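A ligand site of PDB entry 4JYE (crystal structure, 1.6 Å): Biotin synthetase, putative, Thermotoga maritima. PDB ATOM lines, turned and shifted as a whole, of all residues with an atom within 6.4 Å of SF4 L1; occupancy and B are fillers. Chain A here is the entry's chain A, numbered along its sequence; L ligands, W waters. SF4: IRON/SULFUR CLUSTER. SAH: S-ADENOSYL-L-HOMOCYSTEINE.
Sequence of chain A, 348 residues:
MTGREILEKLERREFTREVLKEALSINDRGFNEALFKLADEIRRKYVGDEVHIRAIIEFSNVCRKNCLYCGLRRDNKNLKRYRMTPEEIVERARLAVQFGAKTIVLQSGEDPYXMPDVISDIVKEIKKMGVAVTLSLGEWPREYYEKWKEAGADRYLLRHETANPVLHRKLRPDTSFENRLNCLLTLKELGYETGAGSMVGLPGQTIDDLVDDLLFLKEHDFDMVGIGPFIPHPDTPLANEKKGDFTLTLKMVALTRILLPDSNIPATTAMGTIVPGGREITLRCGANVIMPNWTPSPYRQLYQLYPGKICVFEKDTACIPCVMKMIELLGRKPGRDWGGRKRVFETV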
ATOM      1  N   VAL A  62     -17.362   7.179  -7.409  1.00  0.00           N
ATOM      2  CA  VAL A  62     -15.905   6.957  -7.605  1.00  0.00           C
ATOM      3  C   VAL A  62     -15.563   7.185  -9.077  1.00  0.00           C
ATOM      4  O   VAL A  62     -16.278   6.678  -9.958  1.00  0.00           O
ATOM      5  CB  VAL A  62     -15.497   5.543  -7.150  1.00  0.00           C
ATOM      6  CG1 VAL A  62     -14.031   5.247  -7.554  1.00  0.00           C
ATOM      7  CG2 VAL A  62     -15.725   5.402  -5.642  1.00  0.00           C
ATOM      8  N   CYS A  63     -14.510   7.948  -9.371  1.00  0.00           N
ATOM      9  CA  CYS A  63     -14.084   8.112 -10.758  1.00  0.00           C
ATOM     10  C   CYS A  63     -12.570   8.144 -10.896  1.00  0.00           C
ATOM     11  O   CYS A  63     -11.869   8.773 -10.071  1.00  0.00           O
ATOM     12  CB  CYS A  63     -14.700   9.349 -11.440  1.00  0.00           C
ATOM     13  SG  CYS A  63     -14.546   9.337 -13.244  1.00  0.00           S
ATOM     14  N   ARG A  64     -12.087   7.432 -11.922  1.00  0.00           N
ATOM     15  CA  ARG A  64     -10.665   7.456 -12.304  1.00  0.00           C
ATOM     16  C   ARG A  64     -10.254   8.641 -13.213  1.00  0.00           C
ATOM     17  O   ARG A  64      -9.047   8.862 -13.413  1.00  0.00           O
ATOM     18  CB  ARG A  64     -10.299   6.183 -13.046  1.00  0.00           C
ATOM     19  CG  ARG A  64     -10.947   6.005 -14.402  1.00  0.00           C
ATOM     20  CD  ARG A  64     -10.711   4.675 -15.008  1.00  0.00           C
ATOM     21  NE  ARG A  64     -11.399   4.567 -16.303  1.00  0.00           N
ATOM     22  CZ  ARG A  64     -11.206   3.600 -17.183  1.00  0.00           C
ATOM     23  NH1 ARG A  64     -10.345   2.627 -16.931  1.00  0.00           N
ATOM     24  NH2 ARG A  64     -11.883   3.597 -18.322  1.00  0.00           N
ATOM     25  N   LYS A  65     -11.227   9.297 -13.861  1.00  0.00           N
ATOM     26  CA  LYS A  65     -10.908  10.401 -14.782  1.00  0.00           C
ATOM     27  C   LYS A  65     -10.876  11.743 -14.039  1.00  0.00           C
ATOM     28  O   LYS A  65     -11.233  11.821 -12.859  1.00  0.00           O
ATOM     29  CB  LYS A  65     -11.858  10.405 -15.987  1.00  0.00           C
ATOM     30  CG  LYS A  65     -11.496   9.395 -17.069  1.00  0.00           C
ATOM     31  CD  LYS A  65     -12.346   9.591 -18.320  1.00  0.00           C
ATOM     32  CE  LYS A  65     -11.824   8.843 -19.541  1.00  0.00           C
ATOM     33  NZ  LYS A  65     -11.582   7.390 -19.286  1.00  0.00           N
ATOM     34  N   ASN A  66     -10.362  12.775 -14.705  1.00  0.00           N
ATOM     35  CA  ASN A  66     -10.098  14.049 -14.074  1.00  0.00           C
ATOM     36  C   ASN A  66     -10.701  15.200 -14.893  1.00  0.00           C
ATOM     37  O   ASN A  66     -10.119  16.277 -15.005  1.00  0.00           O
ATOM     38  CB  ASN A  66      -8.575  14.227 -13.884  1.00  0.00           C
ATOM     39  CG  ASN A  66      -8.217  15.059 -12.694  1.00  0.00           C
ATOM     40  OD1 ASN A  66      -8.970  15.153 -11.708  1.00  0.00           O
ATOM     41  ND2 ASN A  66      -7.001  15.614 -12.720  1.00  0.00           N
ATOM     42  N   CYS A  67     -11.883  14.970 -15.444  1.00  0.00           N
ATOM     43  CA  CYS A  67     -12.545  15.994 -16.298  1.00  0.00           C
ATOM     44  C   CYS A  67     -12.601  17.329 -15.584  1.00  0.00           C
ATOM     45  O   CYS A  67     -12.962  17.365 -14.403  1.00  0.00           O
ATOM     46  CB  CYS A  67     -13.938  15.531 -16.758  1.00  0.00           C
ATOM     47  SG  CYS A  67     -13.903  13.957 -17.611  1.00  0.00           S
ATOM     48  N   LEU A  68     -12.252  18.423 -16.277  1.00  0.00           N
ATOM     49  CA  LEU A  68     -12.039  19.731 -15.611  1.00  0.00           C
ATOM     50  C   LEU A  68     -13.317  20.348 -15.047  1.00  0.00           C
ATOM     51  O   LEU A  68     -13.284  21.102 -14.086  1.00  0.00           O
ATOM     52  CB  LEU A  68     -11.309  20.740 -16.519  1.00  0.00           C
ATOM     53  CG  LEU A  68      -9.771  20.826 -16.327  1.00  0.00           C
ATOM     54  CD1 LEU A  68      -9.070  19.498 -16.553  1.00  0.00           C
ATOM     55  CD2 LEU A  68      -9.175  21.926 -17.249  1.00  0.00           C
ATOM     56  N   TYR A  69     -14.456  19.960 -15.614  1.00  0.00           N
ATOM     57  CA  TYR A  69     -15.747  20.532 -15.255  1.00  0.00           C
ATOM     58  C   TYR A  69     -16.495  19.788 -14.178  1.00  0.00           C
ATOM     59  O   TYR A  69     -17.505  20.325 -13.648  1.00  0.00           O
ATOM     60  CB  TYR A  69     -16.663  20.566 -16.516  1.00  0.00           C
ATOM     61  CG  TYR A  69     -16.673  19.298 -17.326  1.00  0.00           C
ATOM     62  CD1 TYR A  69     -17.420  18.178 -16.931  1.00  0.00           C
ATOM     63  CD2 TYR A  69     -15.922  19.185 -18.493  1.00  0.00           C
ATOM     64  CE1 TYR A  69     -17.429  17.016 -17.709  1.00  0.00           C
ATOM     65  CE2 TYR A  69     -15.911  18.039 -19.243  1.00  0.00           C
ATOM     66  CZ  TYR A  69     -16.671  16.960 -18.860  1.00  0.00           C
ATOM     67  OH  TYR A  69     -16.641  15.817 -19.623  1.00  0.00           O
ATOM     68  N   CYS A  70     -16.024  18.586 -13.822  1.00  0.00           N
ATOM     69  CA  CYS A  70     -16.836  17.630 -13.047  1.00  0.00           C
ATOM     70  C   CYS A  70     -16.443  17.530 -11.589  1.00  0.00           C
ATOM     71  O   CYS A  70     -15.269  17.263 -11.277  1.00  0.00           O
ATOM     72  CB  CYS A  70     -16.724  16.249 -13.665  1.00  0.00           C
ATOM     73  SG  CYS A  70     -17.865  15.058 -12.975  1.00  0.00           S
ATOM     74  N   GLY A  71     -17.419  17.657 -10.693  1.00  0.00           N
ATOM     75  CA  GLY A  71     -17.203  17.501  -9.278  1.00  0.00           C
ATOM     76  C   GLY A  71     -16.731  16.123  -8.850  1.00  0.00           C
ATOM     77  O   GLY A  71     -16.143  15.994  -7.776  1.00  0.00           O
ATOM     78  N   LEU A  72     -16.981  15.083  -9.652  1.00  0.00           N
ATOM     79  CA  LEU A  72     -16.495  13.730  -9.305  1.00  0.00           C
ATOM     80  C   LEU A  72     -15.032  13.479  -9.737  1.00  0.00           C
ATOM     81  O   LEU A  72     -14.498  12.406  -9.473  1.00  0.00           O
ATOM     82  CB  LEU A  72     -17.363  12.622  -9.907  1.00  0.00           C
ATOM     83  CG  LEU A  72     -18.867  12.646  -9.577  1.00  0.00           C
ATOM     84  CD1 LEU A  72     -19.479  11.286  -9.876  1.00  0.00           C
ATOM     85  CD2 LEU A  72     -19.267  13.126  -8.205  1.00  0.00           C
ATOM     86  N   ARG A  73     -14.401  14.455 -10.416  1.00  0.00           N
ATOM     87  CA  ARG A  73     -13.031  14.289 -10.935  1.00  0.00           C
ATOM     88  C   ARG A  73     -12.092  13.738  -9.851  1.00  0.00           C
ATOM     89  O   ARG A  73     -12.240  14.045  -8.681  1.00  0.00           O
ATOM     90  CB  ARG A  73     -12.509  15.617 -11.493  1.00  0.00           C
ATOM     91  CG  ARG A  73     -12.261  16.704 -10.436  1.00  0.00           C
ATOM     92  CD  ARG A  73     -12.086  18.056 -11.112  1.00  0.00           C
ATOM     93  NE  ARG A  73     -11.121  18.014 -12.198  1.00  0.00           N
ATOM     94  CZ  ARG A  73      -9.814  18.331 -12.074  1.00  0.00           C
ATOM     95  NH1 ARG A  73      -9.312  18.681 -10.902  1.00  0.00           N
ATOM     96  NH2 ARG A  73      -9.017  18.257 -13.113  1.00  0.00           N
ATOM     97  N   ARG A  74     -11.129  12.911 -10.240  1.00  0.00           N
ATOM     98  CA  ARG A  74     -10.376  12.175  -9.220  1.00  0.00           C
ATOM     99  C   ARG A  74      -9.596  13.078  -8.272  1.00  0.00           C
ATOM    100  O   ARG A  74      -9.393  12.711  -7.106  1.00  0.00           O
ATOM    101  CB  ARG A  74      -9.465  11.123  -9.834  1.00  0.00           C
ATOM    102  CG  ARG A  74      -8.390  11.637 -10.668  1.00  0.00           C
ATOM    103  CD  ARG A  74      -7.298  10.591 -11.011  1.00  0.00           C
ATOM    104  NE  ARG A  74      -6.289  11.323 -11.760  1.00  0.00           N
ATOM    105  CZ  ARG A  74      -6.238  11.486 -13.075  1.00  0.00           C
ATOM    106  NH1 ARG A  74      -7.104  10.897 -13.908  1.00  0.00           N
ATOM    107  NH2 ARG A  74      -5.283  12.259 -13.602  1.00  0.00           N
ATOM    108  N   SER A 108     -22.775   6.113 -13.182  1.00  0.00           N
ATOM    109  CA  SER A 108     -21.695   6.253 -12.202  1.00  0.00           C
ATOM    110  C   SER A 108     -20.537   7.055 -12.757  1.00  0.00           C
ATOM    111  O   SER A 108     -20.454   7.373 -13.964  1.00  0.00           O
ATOM    112  CB  SER A 108     -21.195   4.858 -11.784  1.00  0.00           C
ATOM    113  OG  SER A 108     -20.613   4.193 -12.896  1.00  0.00           O
ATOM    114  N   GLY A 109     -19.615   7.399 -11.855  1.00  0.00           N
ATOM    115  CA  GLY A 109     -18.281   7.757 -12.296  1.00  0.00           C
ATOM    116  C   GLY A 109     -17.657   6.545 -12.957  1.00  0.00           C
ATOM    117  O   GLY A 109     -18.190   5.417 -12.896  1.00  0.00           O
ATOM    118  N   GLU A 110     -16.532   6.746 -13.621  1.00  0.00           N
ATOM    119  CA  GLU A 110     -15.734   5.642 -14.125  1.00  0.00           C
ATOM    120  C   GLU A 110     -15.034   4.925 -12.990  1.00  0.00           C
ATOM    121  O   GLU A 110     -13.831   5.160 -12.696  1.00  0.00           O
ATOM    122  CB  GLU A 110     -14.747   6.085 -15.199  1.00  0.00           C
ATOM    123  CG  GLU A 110     -15.422   6.577 -16.491  1.00  0.00           C
ATOM    124  CD  GLU A 110     -14.482   6.647 -17.700  1.00  0.00           C
ATOM    125  OE1 GLU A 110     -13.315   6.224 -17.599  1.00  0.00           O
ATOM    126  OE2 GLU A 110     -14.960   7.123 -18.773  1.00  0.00           O
ATOM    127  N   GLY A 138     -19.458   5.683 -18.753  1.00  0.00           N
ATOM    128  CA  GLY A 138     -18.256   6.218 -19.343  1.00  0.00           C
ATOM    129  C   GLY A 138     -17.633   5.347 -20.435  1.00  0.00           C
ATOM    130  O   GLY A 138     -18.307   4.546 -21.088  1.00  0.00           O
ATOM    131  N   GLU A 161     -20.030  15.640 -25.330  1.00  0.00           N
ATOM    132  CA  GLU A 161     -19.537  16.738 -24.479  1.00  0.00           C
ATOM    133  C   GLU A 161     -19.249  18.003 -25.282  1.00  0.00           C
ATOM    134  O   GLU A 161     -19.855  19.056 -25.039  1.00  0.00           O
ATOM    135  CB  GLU A 161     -18.295  16.341 -23.659  1.00  0.00           C
ATOM    136  CG  GLU A 161     -18.399  15.025 -22.840  1.00  0.00           C
ATOM    137  CD  GLU A 161     -19.581  14.950 -21.857  1.00  0.00           C
ATOM    138  OE1 GLU A 161     -20.419  15.900 -21.748  1.00  0.00           O
ATOM    139  OE2 GLU A 161     -19.654  13.886 -21.197  1.00  0.00           O
ATOM    140  N   ARG A 172     -10.828  17.250 -20.951  1.00  0.00           N
ATOM    141  CA  ARG A 172     -10.938  15.845 -20.600  1.00  0.00           C
ATOM    142  C   ARG A 172      -9.564  15.224 -20.849  1.00  0.00           C
ATOM    143  O   ARG A 172      -9.367  14.487 -21.825  1.00  0.00           O
ATOM    144  CB  ARG A 172     -12.059  15.177 -21.421  1.00  0.00           C
ATOM    145  CG  ARG A 172     -13.388  15.938 -21.330  1.00  0.00           C
ATOM    146  CD  ARG A 172     -14.547  15.155 -21.902  1.00  0.00           C
ATOM    147  NE  ARG A 172     -14.766  13.986 -21.064  1.00  0.00           N
ATOM    148  CZ  ARG A 172     -14.611  12.724 -21.435  1.00  0.00           C
ATOM    149  NH1 ARG A 172     -14.332  12.395 -22.697  1.00  0.00           N
ATOM    150  NH2 ARG A 172     -14.760  11.767 -20.528  1.00  0.00           N
ATOM    151  N   ARG A 180     -13.936   9.212 -27.603  1.00  0.00           N
ATOM    152  CA  ARG A 180     -15.388   9.338 -27.328  1.00  0.00           C
ATOM    153  C   ARG A 180     -16.233   8.871 -28.502  1.00  0.00           C
ATOM    154  O   ARG A 180     -17.197   8.113 -28.342  1.00  0.00           O
ATOM    155  CB  ARG A 180     -15.744  10.794 -26.980  1.00  0.00           C
ATOM    156  CG  ARG A 180     -16.973  10.963 -26.120  1.00  0.00           C
ATOM    157  CD  ARG A 180     -16.747  10.528 -24.682  1.00  0.00           C
ATOM    158  NE  ARG A 180     -17.896  10.907 -23.852  1.00  0.00           N
ATOM    159  CZ  ARG A 180     -18.046  10.594 -22.565  1.00  0.00           C
ATOM    160  NH1 ARG A 180     -17.104   9.920 -21.927  1.00  0.00           N
ATOM    161  NH2 ARG A 180     -19.149  10.982 -21.895  1.00  0.00           N
ATOM    162  N   TYR A 303     -23.581  12.746  -5.043  1.00  0.00           N
ATOM    163  CA  TYR A 303     -23.374  12.628  -6.471  1.00  0.00           C
ATOM    164  C   TYR A 303     -23.376  14.009  -7.094  1.00  0.00           C
ATOM    165  O   TYR A 303     -24.344  14.428  -7.725  1.00  0.00           O
ATOM    166  CB  TYR A 303     -24.379  11.677  -7.113  1.00  0.00           C
ATOM    167  CG  TYR A 303     -24.001  11.230  -8.504  1.00  0.00           C
ATOM    168  CD1 TYR A 303     -23.093  10.206  -8.704  1.00  0.00           C
ATOM    169  CD2 TYR A 303     -24.598  11.793  -9.618  1.00  0.00           C
ATOM    170  CE1 TYR A 303     -22.745   9.780  -9.979  1.00  0.00           C
ATOM    171  CE2 TYR A 303     -24.273  11.376 -10.893  1.00  0.00           C
ATOM    172  CZ  TYR A 303     -23.375  10.369 -11.073  1.00  0.00           C
ATOM    173  OH  TYR A 303     -23.089   9.996 -12.373  1.00  0.00           O
ATOM    174  N   LEU A 305     -21.907  16.101  -9.619  1.00  0.00           N
ATOM    175  CA  LEU A 305     -21.319  16.511 -10.888  1.00  0.00           C
ATOM    176  C   LEU A 305     -21.182  18.040 -10.906  1.00  0.00           C
ATOM    177  O   LEU A 305     -20.161  18.570 -11.322  1.00  0.00           O
ATOM    178  CB  LEU A 305     -22.209  16.043 -12.065  1.00  0.00           C
ATOM    179  CG  LEU A 305     -22.503  14.546 -12.132  1.00  0.00           C
ATOM    180  CD1 LEU A 305     -23.517  14.304 -13.281  1.00  0.00           C
ATOM    181  CD2 LEU A 305     -21.246  13.714 -12.350  1.00  0.00           C
HETATM  182 FE1  SF4 L   1     -15.519  12.826 -16.225  1.00  0.00          FE
HETATM  183 FE2  SF4 L   1     -17.900  11.268 -16.004  1.00  0.00          FE
HETATM  184 FE3  SF4 L   1     -15.697  11.046 -14.174  1.00  0.00          FE
HETATM  185 FE4  SF4 L   1     -17.194  13.280 -14.162  1.00  0.00          FE
HETATM  186  S1  SF4 L   1     -17.952  11.200 -13.685  1.00  0.00           S
HETATM  187  S2  SF4 L   1     -14.893  13.160 -14.042  1.00  0.00           S
HETATM  188  S3  SF4 L   1     -17.737  13.553 -16.381  1.00  0.00           S
HETATM  189  S4  SF4 L   1     -15.708  10.562 -16.423  1.00  0.00           S
HETATM  190  N   SAH L   2     -18.963   9.219 -15.959  1.00  0.00           N
HETATM  191  CA  SAH L   2     -19.962   9.094 -17.076  1.00  0.00           C
HETATM  192  CB  SAH L   2     -21.375   9.395 -16.522  1.00  0.00           C
HETATM  193  CG  SAH L   2     -21.425  10.470 -15.431  1.00  0.00           C
HETATM  194  SD  SAH L   2     -21.163  12.136 -16.032  1.00  0.00           S
HETATM  195  C   SAH L   2     -19.612  10.021 -18.199  1.00  0.00           C
HETATM  196  O   SAH L   2     -18.699  10.890 -18.074  1.00  0.00           O
HETATM  197  OXT SAH L   2     -20.216   9.874 -19.264  1.00  0.00           O
HETATM  198  C5' SAH L   2     -22.736  12.494 -16.784  1.00  0.00           C
HETATM  199  C4' SAH L   2     -22.807  13.845 -17.534  1.00  0.00           C
HETATM  200  O4' SAH L   2     -22.821  14.916 -16.587  1.00  0.00           O
HETATM  201  C3' SAH L   2     -21.646  14.211 -18.439  1.00  0.00           C
HETATM  202  O3' SAH L   2     -21.708  13.553 -19.717  1.00  0.00           O
HETATM  203  C2' SAH L   2     -21.682  15.741 -18.477  1.00  0.00           C
HETATM  204  O2' SAH L   2     -22.246  16.282 -19.694  1.00  0.00           O
HETATM  205  C1' SAH L   2     -22.532  16.118 -17.260  1.00  0.00           C
HETATM  206  N9  SAH L   2     -21.793  17.032 -16.382  1.00  0.00           N
HETATM  207  C8  SAH L   2     -20.646  16.740 -15.703  1.00  0.00           C
HETATM  208  N7  SAH L   2     -20.180  17.841 -15.045  1.00  0.00           N
HETATM  209  C5  SAH L   2     -21.081  18.835 -15.305  1.00  0.00           C
HETATM  210  C6  SAH L   2     -21.211  20.246 -14.915  1.00  0.00           C
HETATM  211  N6  SAH L   2     -20.267  20.810 -14.100  1.00  0.00           N
HETATM  212  N1  SAH L   2     -22.255  20.968 -15.428  1.00  0.00           N
HETATM  213  C2  SAH L   2     -23.210  20.397 -16.203  1.00  0.00           C
HETATM  214  N3  SAH L   2     -23.153  19.106 -16.590  1.00  0.00           N
HETATM  215  C4  SAH L   2     -22.128  18.313 -16.196  1.00  0.00           C
HETATM  216  O   HOH W   1     -16.542   9.242 -19.315  1.00  0.00           O
HETATM  217  O   HOH W   2     -17.599  13.238 -19.675  1.00  0.00           O
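FE2 of SF4 L1 is bound by O of SAH L2.
Water W1 lies within hydrogen-bond range of the side-chain carboxylate of Glu 110 (2.7 Å), the guanidinium group of Arg 180 (2.8 Å), a sulfur (S4) of SF4 L1 (3.3 Å) and the guanidinium group of Arg 172 (3.3 Å).
Water W2 lies within hydrogen-bond range of the side-chain carboxylate of Glu 161, the side-chain hydroxyl of Tyr 69, the guanidinium group of Arg 172 and a sulfur (S3) of SF4 L1.
The backbone carbonyl oxygen of Cys 67 lies within hydrogen-bond range of the guanidinium group of Arg 73, at 2.9 Å.
The backbone NH (N) of Leu 72 sits close to the side-chain sulfur (SG) of Cys 70, 3.4 Å away.
The guanidinium group (NH2) of Arg 73 sits at hydrogen-bond distance from the backbone carbonyl oxygen (O) of Asn 66, 3.0 Å away.
The side-chain sulfur of Cys 67 lies close to the guanidinium group of Arg 172 (3.6 Å).
NE of Arg 64 is in salt-bridge range of OE1 of Glu 110 (2.8 Å).
N of Arg 74 lies within hydrogen-bond range of O of Lys 65, at 2.8 Å.
N of Lys 65 sits close to SG of Cys 63, 3.4 Å away.
N of Glu 110 sits close to SG of Cys 63.
Residues that only touch SF4 L1: Lys 65 (3.9 Å), Tyr 69 (3.7 Å), Arg 73 (3.8 Å), Gly 109 (3.7 Å) and Glu 110 (3.996 Å).
Within 4 Å of SF4 L1: Cys 63, Lys 65, Cys 67, Tyr 69, Cys 70, Arg 73, Gly 109 and Glu 110.
The nearest printed residue that does not touch SF4 L1 is Leu 72 (4.1 Å).
A nitrogen (N) of SAH L2 sits close to the backbone carbonyl oxygen (O) of Ser 108.
The guanidinium group of Arg 180 is in salt-bridge range of an oxygen (OXT) of SAH L2 (3.0 Å).
The backbone NH (N) of Cys 67 lies close to a sulfur (S2) of SF4 L1.
The side-chain carboxylate (OE2) of Glu 161 is in hydrogen-bond range of an oxygen (O3') of SAH L2 (2.6 Å).
The side-chain sulfur (SG) of Cys 67 binds an iron atom (FE1) of SF4 L1 (2.4 Å).
An iron atom (FE4) of SF4 L1 is bound by the side-chain sulfur of Cys 70 (2.2 Å).
N6 of SAH L2 is in hydrogen-bond range of O of Tyr 69, at 2.8 Å.
An iron atom (FE3) of SF4 L1 is bound by the side-chain sulfur (SG) of Cys 63 (2.3 Å).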
